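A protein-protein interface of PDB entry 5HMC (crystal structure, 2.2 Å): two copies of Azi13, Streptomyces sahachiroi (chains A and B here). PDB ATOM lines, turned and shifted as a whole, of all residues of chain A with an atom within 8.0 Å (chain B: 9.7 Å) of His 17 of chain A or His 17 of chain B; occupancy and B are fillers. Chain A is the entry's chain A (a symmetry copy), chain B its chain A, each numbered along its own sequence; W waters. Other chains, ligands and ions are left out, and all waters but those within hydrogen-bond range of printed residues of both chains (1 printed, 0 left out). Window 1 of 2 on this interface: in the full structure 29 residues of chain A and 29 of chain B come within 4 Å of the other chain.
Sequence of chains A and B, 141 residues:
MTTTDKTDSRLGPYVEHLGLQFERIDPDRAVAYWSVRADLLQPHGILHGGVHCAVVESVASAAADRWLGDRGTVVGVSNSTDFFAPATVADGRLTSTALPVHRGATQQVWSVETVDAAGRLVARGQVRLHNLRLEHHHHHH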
ATOM      1  N   GLY A  12      12.750  -2.369  24.311  1.00  0.00           N
ATOM      2  CA  GLY A  12      12.861  -1.590  23.109  1.00  0.00           C
ATOM      3  C   GLY A  12      11.653  -1.766  22.216  1.00  0.00           C
ATOM      4  O   GLY A  12      10.834  -2.671  22.393  1.00  0.00           O
ATOM      5  N   PRO A  13      11.526  -0.883  21.227  1.00  0.00           N
ATOM      6  CA  PRO A  13      10.339  -0.926  20.365  1.00  0.00           C
ATOM      7  C   PRO A  13      10.354  -2.067  19.361  1.00  0.00           C
ATOM      8  O   PRO A  13       9.278  -2.540  18.981  1.00  0.00           O
ATOM      9  CB  PRO A  13      10.379   0.437  19.662  1.00  0.00           C
ATOM     10  CG  PRO A  13      11.843   0.798  19.648  1.00  0.00           C
ATOM     11  CD  PRO A  13      12.383   0.284  20.953  1.00  0.00           C
ATOM     12  N   TYR A  14      11.526  -2.504  18.892  1.00  0.00           N
ATOM     13  CA  TYR A  14      11.543  -3.576  17.906  1.00  0.00           C
ATOM     14  C   TYR A  14      11.098  -4.887  18.525  1.00  0.00           C
ATOM     15  O   TYR A  14      10.398  -5.670  17.881  1.00  0.00           O
ATOM     16  CB  TYR A  14      12.926  -3.733  17.277  1.00  0.00           C
ATOM     17  CG  TYR A  14      12.887  -4.549  16.005  1.00  0.00           C
ATOM     18  CD1 TYR A  14      12.184  -4.098  14.888  1.00  0.00           C
ATOM     19  CD2 TYR A  14      13.532  -5.777  15.917  1.00  0.00           C
ATOM     20  CE1 TYR A  14      12.130  -4.853  13.709  1.00  0.00           C
ATOM     21  CE2 TYR A  14      13.481  -6.539  14.742  1.00  0.00           C
ATOM     22  CZ  TYR A  14      12.783  -6.070  13.643  1.00  0.00           C
ATOM     23  N   VAL A  15      11.468  -5.132  19.782  1.00  0.00           N
ATOM     24  CA  VAL A  15      10.998  -6.345  20.440  1.00  0.00           C
ATOM     25  C   VAL A  15       9.476  -6.343  20.541  1.00  0.00           C
ATOM     26  O   VAL A  15       8.823  -7.361  20.275  1.00  0.00           O
ATOM     27  CB  VAL A  15      11.663  -6.512  21.812  1.00  0.00           C
ATOM     28  CG1 VAL A  15      11.032  -7.679  22.555  1.00  0.00           C
ATOM     29  CG2 VAL A  15      13.142  -6.756  21.631  1.00  0.00           C
ATOM     30  N   GLU A  16       8.883  -5.198  20.891  1.00  0.00           N
ATOM     31  CA  GLU A  16       7.426  -5.113  20.927  1.00  0.00           C
ATOM     32  C   GLU A  16       6.822  -5.405  19.552  1.00  0.00           C
ATOM     33  O   GLU A  16       5.859  -6.171  19.438  1.00  0.00           O
ATOM     34  CB  GLU A  16       6.983  -3.739  21.445  1.00  0.00           C
ATOM     35  N   HIS A  17       7.382  -4.823  18.486  1.00  0.00           N
ATOM     36  CA  HIS A  17       6.822  -5.067  17.155  1.00  0.00           C
ATOM     37  C   HIS A  17       6.899  -6.541  16.760  1.00  0.00           C
ATOM     38  O   HIS A  17       6.014  -7.048  16.055  1.00  0.00           O
ATOM     39  CB  HIS A  17       7.538  -4.212  16.117  1.00  0.00           C
ATOM     40  CG  HIS A  17       7.338  -4.686  14.711  1.00  0.00           C
ATOM     41  ND1 HIS A  17       6.198  -4.410  13.986  1.00  0.00           N
ATOM     42  CD2 HIS A  17       8.135  -5.416  13.894  1.00  0.00           C
ATOM     43  CE1 HIS A  17       6.303  -4.945  12.783  1.00  0.00           C
ATOM     44  NE2 HIS A  17       7.470  -5.560  12.702  1.00  0.00           N
ATOM     45  N   LEU A  18       7.946  -7.244  17.193  1.00  0.00           N
ATOM     46  CA  LEU A  18       8.000  -8.679  16.961  1.00  0.00           C
ATOM     47  C   LEU A  18       6.862  -9.408  17.654  1.00  0.00           C
ATOM     48  O   LEU A  18       6.510 -10.516  17.243  1.00  0.00           O
ATOM     49  CB  LEU A  18       9.338  -9.243  17.437  1.00  0.00           C
ATOM     50  CG  LEU A  18      10.541  -8.833  16.587  1.00  0.00           C
ATOM     51  CD1 LEU A  18      11.829  -9.366  17.194  1.00  0.00           C
ATOM     52  CD2 LEU A  18      10.401  -9.283  15.132  1.00  0.00           C
ATOM     53  N   GLY A  19       6.276  -8.816  18.689  1.00  0.00           N
ATOM     54  CA  GLY A  19       5.230  -9.494  19.421  1.00  0.00           C
ATOM     55  C   GLY A  19       5.722 -10.477  20.453  1.00  0.00           C
ATOM     56  O   GLY A  19       4.963 -11.358  20.869  1.00  0.00           O
ATOM     57  N   LEU A  20       6.973 -10.362  20.885  1.00  0.00           N
ATOM     58  CA  LEU A  20       7.476 -11.285  21.887  1.00  0.00           C
ATOM     59  C   LEU A  20       6.849 -10.977  23.235  1.00  0.00           C
ATOM     60  O   LEU A  20       6.638  -9.818  23.593  1.00  0.00           O
ATOM     61  CB  LEU A  20       8.996 -11.204  21.989  1.00  0.00           C
ATOM     62  CG  LEU A  20       9.775 -11.734  20.793  1.00  0.00           C
ATOM     63  CD1 LEU A  20      11.248 -11.488  20.988  1.00  0.00           C
ATOM     64  CD2 LEU A  20       9.517 -13.216  20.637  1.00  0.00           C
ATOM     65  N   SER A  35       4.141 -15.546  17.746  1.00  0.00           N
ATOM     66  CA  SER A  35       3.371 -16.201  16.709  1.00  0.00           C
ATOM     67  C   SER A  35       3.685 -15.571  15.360  1.00  0.00           C
ATOM     68  O   SER A  35       3.973 -14.374  15.272  1.00  0.00           O
ATOM     69  CB  SER A  35       1.874 -16.092  16.997  1.00  0.00           C
ATOM     70  OG  SER A  35       1.143 -16.280  15.794  1.00  0.00           O
ATOM     71  N   ARG A  37       2.656 -13.848  12.093  1.00  0.00           N
ATOM     72  CA  ARG A  37       1.583 -12.923  11.781  1.00  0.00           C
ATOM     73  C   ARG A  37       1.745 -12.529  10.334  1.00  0.00           C
ATOM     74  O   ARG A  37       2.851 -12.583   9.792  1.00  0.00           O
ATOM     75  CB  ARG A  37       1.605 -11.648  12.652  1.00  0.00           C
ATOM     76  CG  ARG A  37       1.560 -11.864  14.154  1.00  0.00           C
ATOM     77  CD  ARG A  37       1.370 -10.518  14.866  1.00  0.00           C
ATOM     78  NE  ARG A  37       2.213  -9.483  14.272  1.00  0.00           N
ATOM     79  CZ  ARG A  37       3.266  -8.923  14.866  1.00  0.00           C
ATOM     80  NH1 ARG A  37       3.618  -9.269  16.098  1.00  0.00           N
ATOM     81  NH2 ARG A  37       3.967  -8.006  14.219  1.00  0.00           N
ATOM     82  N   ASP A  39       1.897  -9.789   8.846  1.00  0.00           N
ATOM     83  CA  ASP A  39       2.854  -8.727   8.556  1.00  0.00           C
ATOM     84  C   ASP A  39       4.304  -9.188   8.658  1.00  0.00           C
ATOM     85  O   ASP A  39       5.198  -8.438   8.264  1.00  0.00           O
ATOM     86  CB  ASP A  39       2.616  -7.522   9.485  1.00  0.00           C
ATOM     87  CG  ASP A  39       2.780  -7.862  10.952  1.00  0.00           C
ATOM     88  OD1 ASP A  39       2.002  -8.697  11.457  1.00  0.00           O
ATOM     89  OD2 ASP A  39       3.677  -7.284  11.614  1.00  0.00           O
ATOM     90  N   LEU A  40       4.552 -10.403   9.145  1.00  0.00           N
ATOM     91  CA  LEU A  40       5.894 -10.930   9.341  1.00  0.00           C
ATOM     92  C   LEU A  40       6.333 -11.874   8.231  1.00  0.00           C
ATOM     93  O   LEU A  40       7.359 -12.543   8.376  1.00  0.00           O
ATOM     94  CB  LEU A  40       5.980 -11.653  10.691  1.00  0.00           C
ATOM     95  CG  LEU A  40       5.699 -10.808  11.931  1.00  0.00           C
ATOM     96  CD1 LEU A  40       5.903 -11.611  13.206  1.00  0.00           C
ATOM     97  CD2 LEU A  40       6.582  -9.557  11.928  1.00  0.00           C
ATOM     98  N   VAL A  51      12.979 -12.712  10.694  1.00  0.00           N
ATOM     99  CA  VAL A  51      12.214 -12.649  11.937  1.00  0.00           C
ATOM    100  C   VAL A  51      12.750 -13.663  12.947  1.00  0.00           C
ATOM    101  O   VAL A  51      12.885 -13.357  14.137  1.00  0.00           O
ATOM    102  CB  VAL A  51      10.711 -12.849  11.659  1.00  0.00           C
ATOM    103  CG1 VAL A  51       9.919 -12.875  12.970  1.00  0.00           C
ATOM    104  CG2 VAL A  51      10.195 -11.742  10.758  1.00  0.00           C
ATOM    105  N   LEU B  11       7.964  -8.172  -2.471  1.00  0.00           N
ATOM    106  CA  LEU B  11       8.927  -8.755  -1.549  1.00  0.00           C
ATOM    107  C   LEU B  11       8.325  -9.117  -0.205  1.00  0.00           C
ATOM    108  O   LEU B  11       9.031  -9.672   0.645  1.00  0.00           O
ATOM    109  CB  LEU B  11      10.102  -7.798  -1.338  1.00  0.00           C
ATOM    110  CG  LEU B  11      11.040  -7.794  -2.536  1.00  0.00           C
ATOM    111  CD1 LEU B  11      12.126  -6.782  -2.317  1.00  0.00           C
ATOM    112  CD2 LEU B  11      11.619  -9.193  -2.763  1.00  0.00           C
ATOM    113  N   GLY B  12       7.048  -8.829   0.012  1.00  0.00           N
ATOM    114  CA  GLY B  12       6.391  -9.203   1.233  1.00  0.00           C
ATOM    115  C   GLY B  12       6.256  -8.028   2.176  1.00  0.00           C
ATOM    116  O   GLY B  12       6.879  -6.977   2.006  1.00  0.00           O
ATOM    117  N   PRO B  13       5.422  -8.196   3.201  1.00  0.00           N
ATOM    118  CA  PRO B  13       5.164  -7.078   4.116  1.00  0.00           C
ATOM    119  C   PRO B  13       6.308  -6.799   5.077  1.00  0.00           C
ATOM    120  O   PRO B  13       6.470  -5.647   5.491  1.00  0.00           O
ATOM    121  CB  PRO B  13       3.905  -7.534   4.864  1.00  0.00           C
ATOM    122  CG  PRO B  13       3.979  -9.040   4.821  1.00  0.00           C
ATOM    123  CD  PRO B  13       4.564  -9.362   3.474  1.00  0.00           C
ATOM    124  N   TYR B  14       7.083  -7.811   5.475  1.00  0.00           N
ATOM    125  CA  TYR B  14       8.162  -7.553   6.420  1.00  0.00           C
ATOM    126  C   TYR B  14       9.259  -6.728   5.776  1.00  0.00           C
ATOM    127  O   TYR B  14       9.838  -5.855   6.425  1.00  0.00           O
ATOM    128  CB  TYR B  14       8.738  -8.853   6.977  1.00  0.00           C
ATOM    129  CG  TYR B  14       9.568  -8.625   8.220  1.00  0.00           C
ATOM    130  CD1 TYR B  14       8.988  -8.123   9.384  1.00  0.00           C
ATOM    131  CD2 TYR B  14      10.932  -8.892   8.233  1.00  0.00           C
ATOM    132  CE1 TYR B  14       9.750  -7.895  10.536  1.00  0.00           C
ATOM    133  CE2 TYR B  14      11.702  -8.665   9.381  1.00  0.00           C
ATOM    134  CZ  TYR B  14      11.106  -8.170  10.528  1.00  0.00           C
ATOM    135  N   VAL B  15       9.540  -6.966   4.495  1.00  0.00           N
ATOM    136  CA  VAL B  15      10.534  -6.143   3.819  1.00  0.00           C
ATOM    137  C   VAL B  15      10.091  -4.685   3.790  1.00  0.00           C
ATOM    138  O   VAL B  15      10.891  -3.775   4.050  1.00  0.00           O
ATOM    139  CB  VAL B  15      10.819  -6.683   2.411  1.00  0.00           C
ATOM    140  CG1 VAL B  15      11.720  -5.717   1.658  1.00  0.00           C
ATOM    141  CG2 VAL B  15      11.485  -8.035   2.513  1.00  0.00           C
ATOM    142  N   GLU B  16       8.809  -4.435   3.509  1.00  0.00           N
ATOM    143  CA  GLU B  16       8.309  -3.064   3.545  1.00  0.00           C
ATOM    144  C   GLU B  16       8.481  -2.450   4.937  1.00  0.00           C
ATOM    145  O   GLU B  16       8.943  -1.311   5.069  1.00  0.00           O
ATOM    146  CB  GLU B  16       6.842  -3.018   3.098  1.00  0.00           C
ATOM    147  N   HIS B  17       8.135  -3.191   5.994  1.00  0.00           N
ATOM    148  CA  HIS B  17       8.271  -2.632   7.341  1.00  0.00           C
ATOM    149  C   HIS B  17       9.722  -2.295   7.679  1.00  0.00           C
ATOM    150  O   HIS B  17       9.987  -1.327   8.408  1.00  0.00           O
ATOM    151  CB  HIS B  17       7.707  -3.600   8.373  1.00  0.00           C
ATOM    152  CG  HIS B  17       8.170  -3.322   9.770  1.00  0.00           C
ATOM    153  ND1 HIS B  17       7.614  -2.336  10.558  1.00  0.00           N
ATOM    154  CD2 HIS B  17       9.136  -3.903  10.522  1.00  0.00           C
ATOM    155  CE1 HIS B  17       8.213  -2.325  11.734  1.00  0.00           C
ATOM    156  NE2 HIS B  17       9.139  -3.267  11.738  1.00  0.00           N
ATOM    157  N   LEU B  18      10.674  -3.078   7.173  1.00  0.00           N
ATOM    158  CA  LEU B  18      12.074  -2.725   7.351  1.00  0.00           C
ATOM    159  C   LEU B  18      12.413  -1.401   6.688  1.00  0.00           C
ATOM    160  O   LEU B  18      13.390  -0.759   7.076  1.00  0.00           O
ATOM    161  CB  LEU B  18      12.974  -3.825   6.792  1.00  0.00           C
ATOM    162  CG  LEU B  18      12.967  -5.125   7.598  1.00  0.00           C
ATOM    163  CD1 LEU B  18      13.818  -6.182   6.912  1.00  0.00           C
ATOM    164  CD2 LEU B  18      13.427  -4.913   9.042  1.00  0.00           C
ATOM    165  N   GLY B  19      11.628  -0.974   5.703  1.00  0.00           N
ATOM    166  CA  GLY B  19      11.943   0.248   4.998  1.00  0.00           C
ATOM    167  C   GLY B  19      12.975   0.097   3.910  1.00  0.00           C
ATOM    168  O   GLY B  19      13.581   1.092   3.499  1.00  0.00           O
ATOM    169  N   LEU B  20      13.204  -1.118   3.424  1.00  0.00           N
ATOM    170  CA  LEU B  20      14.183  -1.298   2.367  1.00  0.00           C
ATOM    171  C   LEU B  20      13.644  -0.739   1.061  1.00  0.00           C
ATOM    172  O   LEU B  20      12.458  -0.859   0.755  1.00  0.00           O
ATOM    173  CB  LEU B  20      14.536  -2.771   2.196  1.00  0.00           C
ATOM    174  CG  LEU B  20      15.323  -3.407   3.333  1.00  0.00           C
ATOM    175  CD1 LEU B  20      15.501  -4.880   3.078  1.00  0.00           C
ATOM    176  CD2 LEU B  20      16.676  -2.738   3.449  1.00  0.00           C
ATOM    177  N   GLN B  21      14.523  -0.112   0.293  1.00  0.00           N
ATOM    178  CA  GLN B  21      14.176   0.428  -1.012  1.00  0.00           C
ATOM    179  C   GLN B  21      15.252  -0.047  -1.966  1.00  0.00           C
ATOM    180  O   GLN B  21      16.422   0.325  -1.824  1.00  0.00           O
ATOM    181  CB  GLN B  21      14.081   1.950  -0.974  1.00  0.00           C
ATOM    182  CG  GLN B  21      13.082   2.432   0.062  1.00  0.00           C
ATOM    183  CD  GLN B  21      12.585   3.830  -0.202  1.00  0.00           C
ATOM    184  OE1 GLN B  21      13.181   4.807   0.253  1.00  0.00           O
ATOM    185  NE2 GLN B  21      11.480   3.939  -0.941  1.00  0.00           N
ATOM    186  N   TRP B  34      18.376   1.954   3.140  1.00  0.00           N
ATOM    187  CA  TRP B  34      17.491   2.005   4.295  1.00  0.00           C
ATOM    188  C   TRP B  34      18.149   2.885   5.352  1.00  0.00           C
ATOM    189  O   TRP B  34      19.222   3.456   5.137  1.00  0.00           O
ATOM    190  CB  TRP B  34      17.187   0.606   4.831  1.00  0.00           C
ATOM    191  CG  TRP B  34      18.415  -0.228   5.192  1.00  0.00           C
ATOM    192  CD1 TRP B  34      19.371  -0.715   4.330  1.00  0.00           C
ATOM    193  CD2 TRP B  34      18.778  -0.702   6.499  1.00  0.00           C
ATOM    194  NE1 TRP B  34      20.303  -1.452   5.028  1.00  0.00           N
ATOM    195  CE2 TRP B  34      19.963  -1.457   6.358  1.00  0.00           C
ATOM    196  CE3 TRP B  34      18.215  -0.559   7.776  1.00  0.00           C
ATOM    197  CZ2 TRP B  34      20.598  -2.066   7.451  1.00  0.00           C
ATOM    198  CZ3 TRP B  34      18.843  -1.167   8.858  1.00  0.00           C
ATOM    199  CH2 TRP B  34      20.019  -1.918   8.684  1.00  0.00           C
ATOM    200  N   SER B  35      17.501   2.976   6.509  1.00  0.00           N
ATOM    201  CA  SER B  35      17.957   3.865   7.557  1.00  0.00           C
ATOM    202  C   SER B  35      17.508   3.335   8.911  1.00  0.00           C
ATOM    203  O   SER B  35      16.449   2.711   9.028  1.00  0.00           O
ATOM    204  CB  SER B  35      17.409   5.276   7.344  1.00  0.00           C
ATOM    205  OG  SER B  35      17.437   5.988   8.573  1.00  0.00           O
ATOM    206  N   VAL B  36      18.332   3.588   9.933  1.00  0.00           N
ATOM    207  CA  VAL B  36      17.902   3.350  11.302  1.00  0.00           C
ATOM    208  C   VAL B  36      16.708   4.250  11.586  1.00  0.00           C
ATOM    209  O   VAL B  36      16.663   5.410  11.156  1.00  0.00           O
ATOM    210  CB  VAL B  36      19.053   3.608  12.296  1.00  0.00           C
ATOM    211  CG1 VAL B  36      18.623   3.301  13.720  1.00  0.00           C
ATOM    212  CG2 VAL B  36      20.263   2.775  11.932  1.00  0.00           C
ATOM    213  N   ARG B  37      15.719   3.707  12.282  1.00  0.00           N
ATOM    214  CA  ARG B  37      14.542   4.456  12.677  1.00  0.00           C
ATOM    215  C   ARG B  37      14.280   4.136  14.128  1.00  0.00           C
ATOM    216  O   ARG B  37      14.674   3.075  14.614  1.00  0.00           O
ATOM    217  CB  ARG B  37      13.286   4.099  11.852  1.00  0.00           C
ATOM    218  CG  ARG B  37      13.409   4.257  10.346  1.00  0.00           C
ATOM    219  CD  ARG B  37      12.033   4.076   9.693  1.00  0.00           C
ATOM    220  NE  ARG B  37      11.312   2.949  10.282  1.00  0.00           N
ATOM    221  CZ  ARG B  37      11.050   1.801   9.659  1.00  0.00           C
ATOM    222  NH1 ARG B  37      11.423   1.608   8.399  1.00  0.00           N
ATOM    223  NH2 ARG B  37      10.404   0.844  10.304  1.00  0.00           N
ATOM    224  N   ALA B  38      13.608   5.061  14.814  1.00  0.00           N
ATOM    225  CA  ALA B  38      13.403   4.899  16.249  1.00  0.00           C
ATOM    226  C   ALA B  38      12.672   3.600  16.576  1.00  0.00           C
ATOM    227  O   ALA B  38      12.933   2.986  17.616  1.00  0.00           O
ATOM    228  CB  ALA B  38      12.646   6.106  16.806  1.00  0.00           C
ATOM    229  N   ASP B  39      11.772   3.148  15.703  1.00  0.00           N
ATOM    230  CA  ASP B  39      11.044   1.917  15.984  1.00  0.00           C
ATOM    231  C   ASP B  39      11.896   0.665  15.798  1.00  0.00           C
ATOM    232  O   ASP B  39      11.453  -0.421  16.175  1.00  0.00           O
ATOM    233  CB  ASP B  39       9.778   1.829  15.111  1.00  0.00           C
ATOM    234  CG  ASP B  39      10.081   1.823  13.626  1.00  0.00           C
ATOM    235  OD1 ASP B  39      10.633   2.826  13.130  1.00  0.00           O
ATOM    236  OD2 ASP B  39       9.754   0.821  12.944  1.00  0.00           O
ATOM    237  N   LEU B  40      13.106   0.796  15.256  1.00  0.00           N
ATOM    238  CA  LEU B  40      13.986  -0.330  14.978  1.00  0.00           C
ATOM    239  C   LEU B  40      15.068  -0.516  16.032  1.00  0.00           C
ATOM    240  O   LEU B  40      15.995  -1.301  15.815  1.00  0.00           O
ATOM    241  CB  LEU B  40      14.638  -0.156  13.601  1.00  0.00           C
ATOM    242  CG  LEU B  40      13.690  -0.087  12.406  1.00  0.00           C
ATOM    243  CD1 LEU B  40      14.457  -0.005  11.096  1.00  0.00           C
ATOM    244  CD2 LEU B  40      12.747  -1.293  12.412  1.00  0.00           C
ATOM    245  N   LEU B  41      14.975   0.175  17.161  1.00  0.00           N
ATOM    246  CA  LEU B  41      16.060   0.233  18.127  1.00  0.00           C
ATOM    247  C   LEU B  41      15.899  -0.814  19.214  1.00  0.00           C
ATOM    248  O   LEU B  41      14.792  -1.270  19.512  1.00  0.00           O
ATOM    249  CB  LEU B  41      16.119   1.612  18.788  1.00  0.00           C
ATOM    250  CG  LEU B  41      16.328   2.794  17.856  1.00  0.00           C
ATOM    251  CD1 LEU B  41      16.048   4.090  18.601  1.00  0.00           C
ATOM    252  CD2 LEU B  41      17.744   2.762  17.287  1.00  0.00           C
ATOM    253  N   LEU B  47      20.657   0.340  16.758  1.00  0.00           N
ATOM    254  CA  LEU B  47      19.871  -0.597  15.968  1.00  0.00           C
ATOM    255  C   LEU B  47      19.857  -1.975  16.621  1.00  0.00           C
ATOM    256  O   LEU B  47      20.902  -2.496  17.025  1.00  0.00           O
ATOM    257  CB  LEU B  47      20.437  -0.689  14.559  1.00  0.00           C
ATOM    258  CG  LEU B  47      19.596  -1.533  13.597  1.00  0.00           C
ATOM    259  CD1 LEU B  47      18.230  -0.901  13.402  1.00  0.00           C
ATOM    260  CD2 LEU B  47      20.307  -1.681  12.285  1.00  0.00           C
ATOM    261  N   HIS B  48      18.655  -2.534  16.761  1.00  0.00           N
ATOM    262  CA  HIS B  48      18.469  -3.930  17.149  1.00  0.00           C
ATOM    263  C   HIS B  48      19.207  -4.826  16.159  1.00  0.00           C
ATOM    264  O   HIS B  48      19.074  -4.661  14.946  1.00  0.00           O
ATOM    265  CB  HIS B  48      16.965  -4.236  17.164  1.00  0.00           C
ATOM    266  CG  HIS B  48      16.591  -5.545  17.792  1.00  0.00           C
ATOM    267  ND1 HIS B  48      16.981  -6.761  17.278  1.00  0.00           N
ATOM    268  CD2 HIS B  48      15.816  -5.825  18.867  1.00  0.00           C
ATOM    269  CE1 HIS B  48      16.478  -7.734  18.018  1.00  0.00           C
ATOM    270  NE2 HIS B  48      15.773  -7.192  18.993  1.00  0.00           N
ATOM    271  N   GLY B  50      18.912  -7.882  15.318  1.00  0.00           N
ATOM    272  CA  GLY B  50      18.027  -8.636  14.446  1.00  0.00           C
ATOM    273  C   GLY B  50      17.646  -7.887  13.185  1.00  0.00           C
ATOM    274  O   GLY B  50      17.362  -8.504  12.160  1.00  0.00           O
ATOM    275  N   VAL B  51      17.658  -6.548  13.228  1.00  0.00           N
ATOM    276  CA  VAL B  51      17.319  -5.789  12.026  1.00  0.00           C
ATOM    277  C   VAL B  51      18.395  -5.975  10.956  1.00  0.00           C
ATOM    278  O   VAL B  51      18.084  -6.150   9.773  1.00  0.00           O
ATOM    279  CB  VAL B  51      17.092  -4.304  12.368  1.00  0.00           C
ATOM    280  CG1 VAL B  51      16.828  -3.492  11.096  1.00  0.00           C
ATOM    281  CG2 VAL B  51      15.928  -4.160  13.331  1.00  0.00           C
ATOM    282  N   ALA B  54      17.759  -9.389   9.398  1.00  0.00           N
ATOM    283  CA  ALA B  54      16.609  -9.367   8.504  1.00  0.00           C
ATOM    284  C   ALA B  54      16.917  -8.607   7.219  1.00  0.00           C
ATOM    285  O   ALA B  54      16.461  -8.996   6.139  1.00  0.00           O
ATOM    286  CB  ALA B  54      15.404  -8.762   9.219  1.00  0.00           C
ATOM    287  N   VAL B  55      17.687  -7.520   7.305  1.00  0.00           N
ATOM    288  CA  VAL B  55      18.089  -6.825   6.084  1.00  0.00           C
ATOM    289  C   VAL B  55      18.980  -7.723   5.236  1.00  0.00           C
ATOM    290  O   VAL B  55      18.813  -7.820   4.013  1.00  0.00           O
ATOM    291  CB  VAL B  55      18.793  -5.497   6.426  1.00  0.00           C
ATOM    292  CG1 VAL B  55      19.592  -4.997   5.230  1.00  0.00           C
ATOM    293  CG2 VAL B  55      17.775  -4.461   6.844  1.00  0.00           C
ATOM    294  N   SER B  58      16.877 -10.234   3.585  1.00  0.00           N
ATOM    295  CA  SER B  58      16.009  -9.680   2.549  1.00  0.00           C
ATOM    296  C   SER B  58      16.769  -9.474   1.244  1.00  0.00           C
ATOM    297  O   SER B  58      16.291  -9.846   0.161  1.00  0.00           O
ATOM    298  CB  SER B  58      15.412  -8.354   3.030  1.00  0.00           C
ATOM    299  OG  SER B  58      14.669  -8.497   4.223  1.00  0.00           O
HETATM  300  O   HOH W   1      13.726  -3.508  20.670  1.00  0.00           O
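The backbone NH (N) of Tyr 14 of chain B lies within hydrogen-bond range of the backbone carbonyl oxygen (O) of Asp 39 of chain A (3.4 Å).
The backbone carbonyl oxygen (O) of Asp 39 of chain B sits at hydrogen-bond distance from the backbone NH (N) of Tyr 14 of chain A.
A ring nitrogen (NE2) of His 17 of chain B is in hydrogen-bond range of a ring nitrogen (NE2) of His 17 of chain A (3.0 Å).
The backbone carbonyl oxygen (O) of His 17 of chain B is in hydrogen-bond range of the guanidinium group (NH2) of Arg 37 of chain B (2.9 Å).
The backbone NH of His 48 of chain B lies within hydrogen-bond range of the backbone carbonyl oxygen of Leu 40 of chain B (3.1 Å).
ND1 of His 48 of chain B sits at hydrogen-bond distance from N of Gly 50 of chain B (3.0 Å).
The guanidinium group (NH2) of Arg 37 of chain B is in salt-bridge range of the side-chain carboxylate (OD2) of Asp 39 of chain B (2.7 Å).
Pro 13 of chain A touches Ala 38 of chain B (CG to O, 3.2 Å).
Asp 39 of chain B touches Pro 13 of chain A.
CD of Pro 13 of chain A touches O of Leu 41 of chain B, at 3.2 Å.
Tyr 14 of chain A touches His 17 of chain B (CE1 to NE2, 3.9 Å).
Leu 40 of chain B touches Tyr 14 of chain A.
Leu 41 of chain B touches Tyr 14 of chain A (O to N, 3.5 Å).
His 48 of chain B touches Val 15 of chain A.
O of Asp 39 of chain A touches CG of Pro 13 of chain B (3.7 Å).
Val 51 of chain A touches Tyr 14 of chain B (CG2 to CE2, 3.7 Å).
Of chain B, only Tyr 14 and His 17 come within 4 Å of His 17 of chain A.
His 17 of chain B touches just these residues of chain A: Tyr 14 (3.9 Å) and His 17 (3.0 Å).
No residue of chain A comes within 4 Å of Glu 16 of chain B.
Printed residues of chain B within 4 Å of Asp 39 of chain A: Pro 13 (3.7 Å) and Tyr 14 (3.4 Å).
Printed residues of chain A within 4 Å of Leu 40 of chain B: Tyr 14 (3.8 Å).
Of the printed residues of chain A, Tyr 14 of chain B touches His 17 (3.9 Å), Asp 39 (3.4 Å), Leu 40 (3.8 Å) and Val 51 (3.7 Å).
Val 15 of chain B touches none of the printed residues of chain A.
Val 36 of chain B touches none of the printed residues of chain A.
The nearest residue of chain B that does not touch His 17 of chain A is Asp 39 of chain B (5.4 Å).
Printed residues of chain A that touch a printed residue of chain B: Pro 13, Tyr 14, Val 15, His 17, Asp 39, Leu 40 and Val 51.
Printed residues of chain B that touch a printed residue of chain A: Pro 13, Tyr 14, His 17, Ala 38, Asp 39, Leu 40, Leu 41, His 48 and Val 51.
Hydrophobic or aromatic side chains of chain B that line the printed part of chain A: Pro 13, Tyr 14, His 17, Leu 40, His 48 and Val 51.
Among the printed residues, 16 pairs touch across the chains.
Tyr 14 of chain A touches Asp 39 of chain B, and with the chains exchanged Asp 39 of chain A touches Tyr 14 of chain B.
Tyr 14 of chain A touches Leu 40 of chain B, and with the chains exchanged Leu 40 of chain A touches Tyr 14 of chain B.
His 17 of chain A touches its own counterpart, His 17 of chain B.
Positions printed for both chains: 12, 13, 14, 15, 16, 17, 18, 19, 20, 35, 37, 39, 40 and 51.
Water W1 lies within hydrogen-bond range of the backbone carbonyl oxygen of Leu 41 of chain B, the backbone NH of Val 15 of chain A, the backbone NH of Tyr 14 of chain A and the backbone carbonyl oxygen of Gly 12 of chain A.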
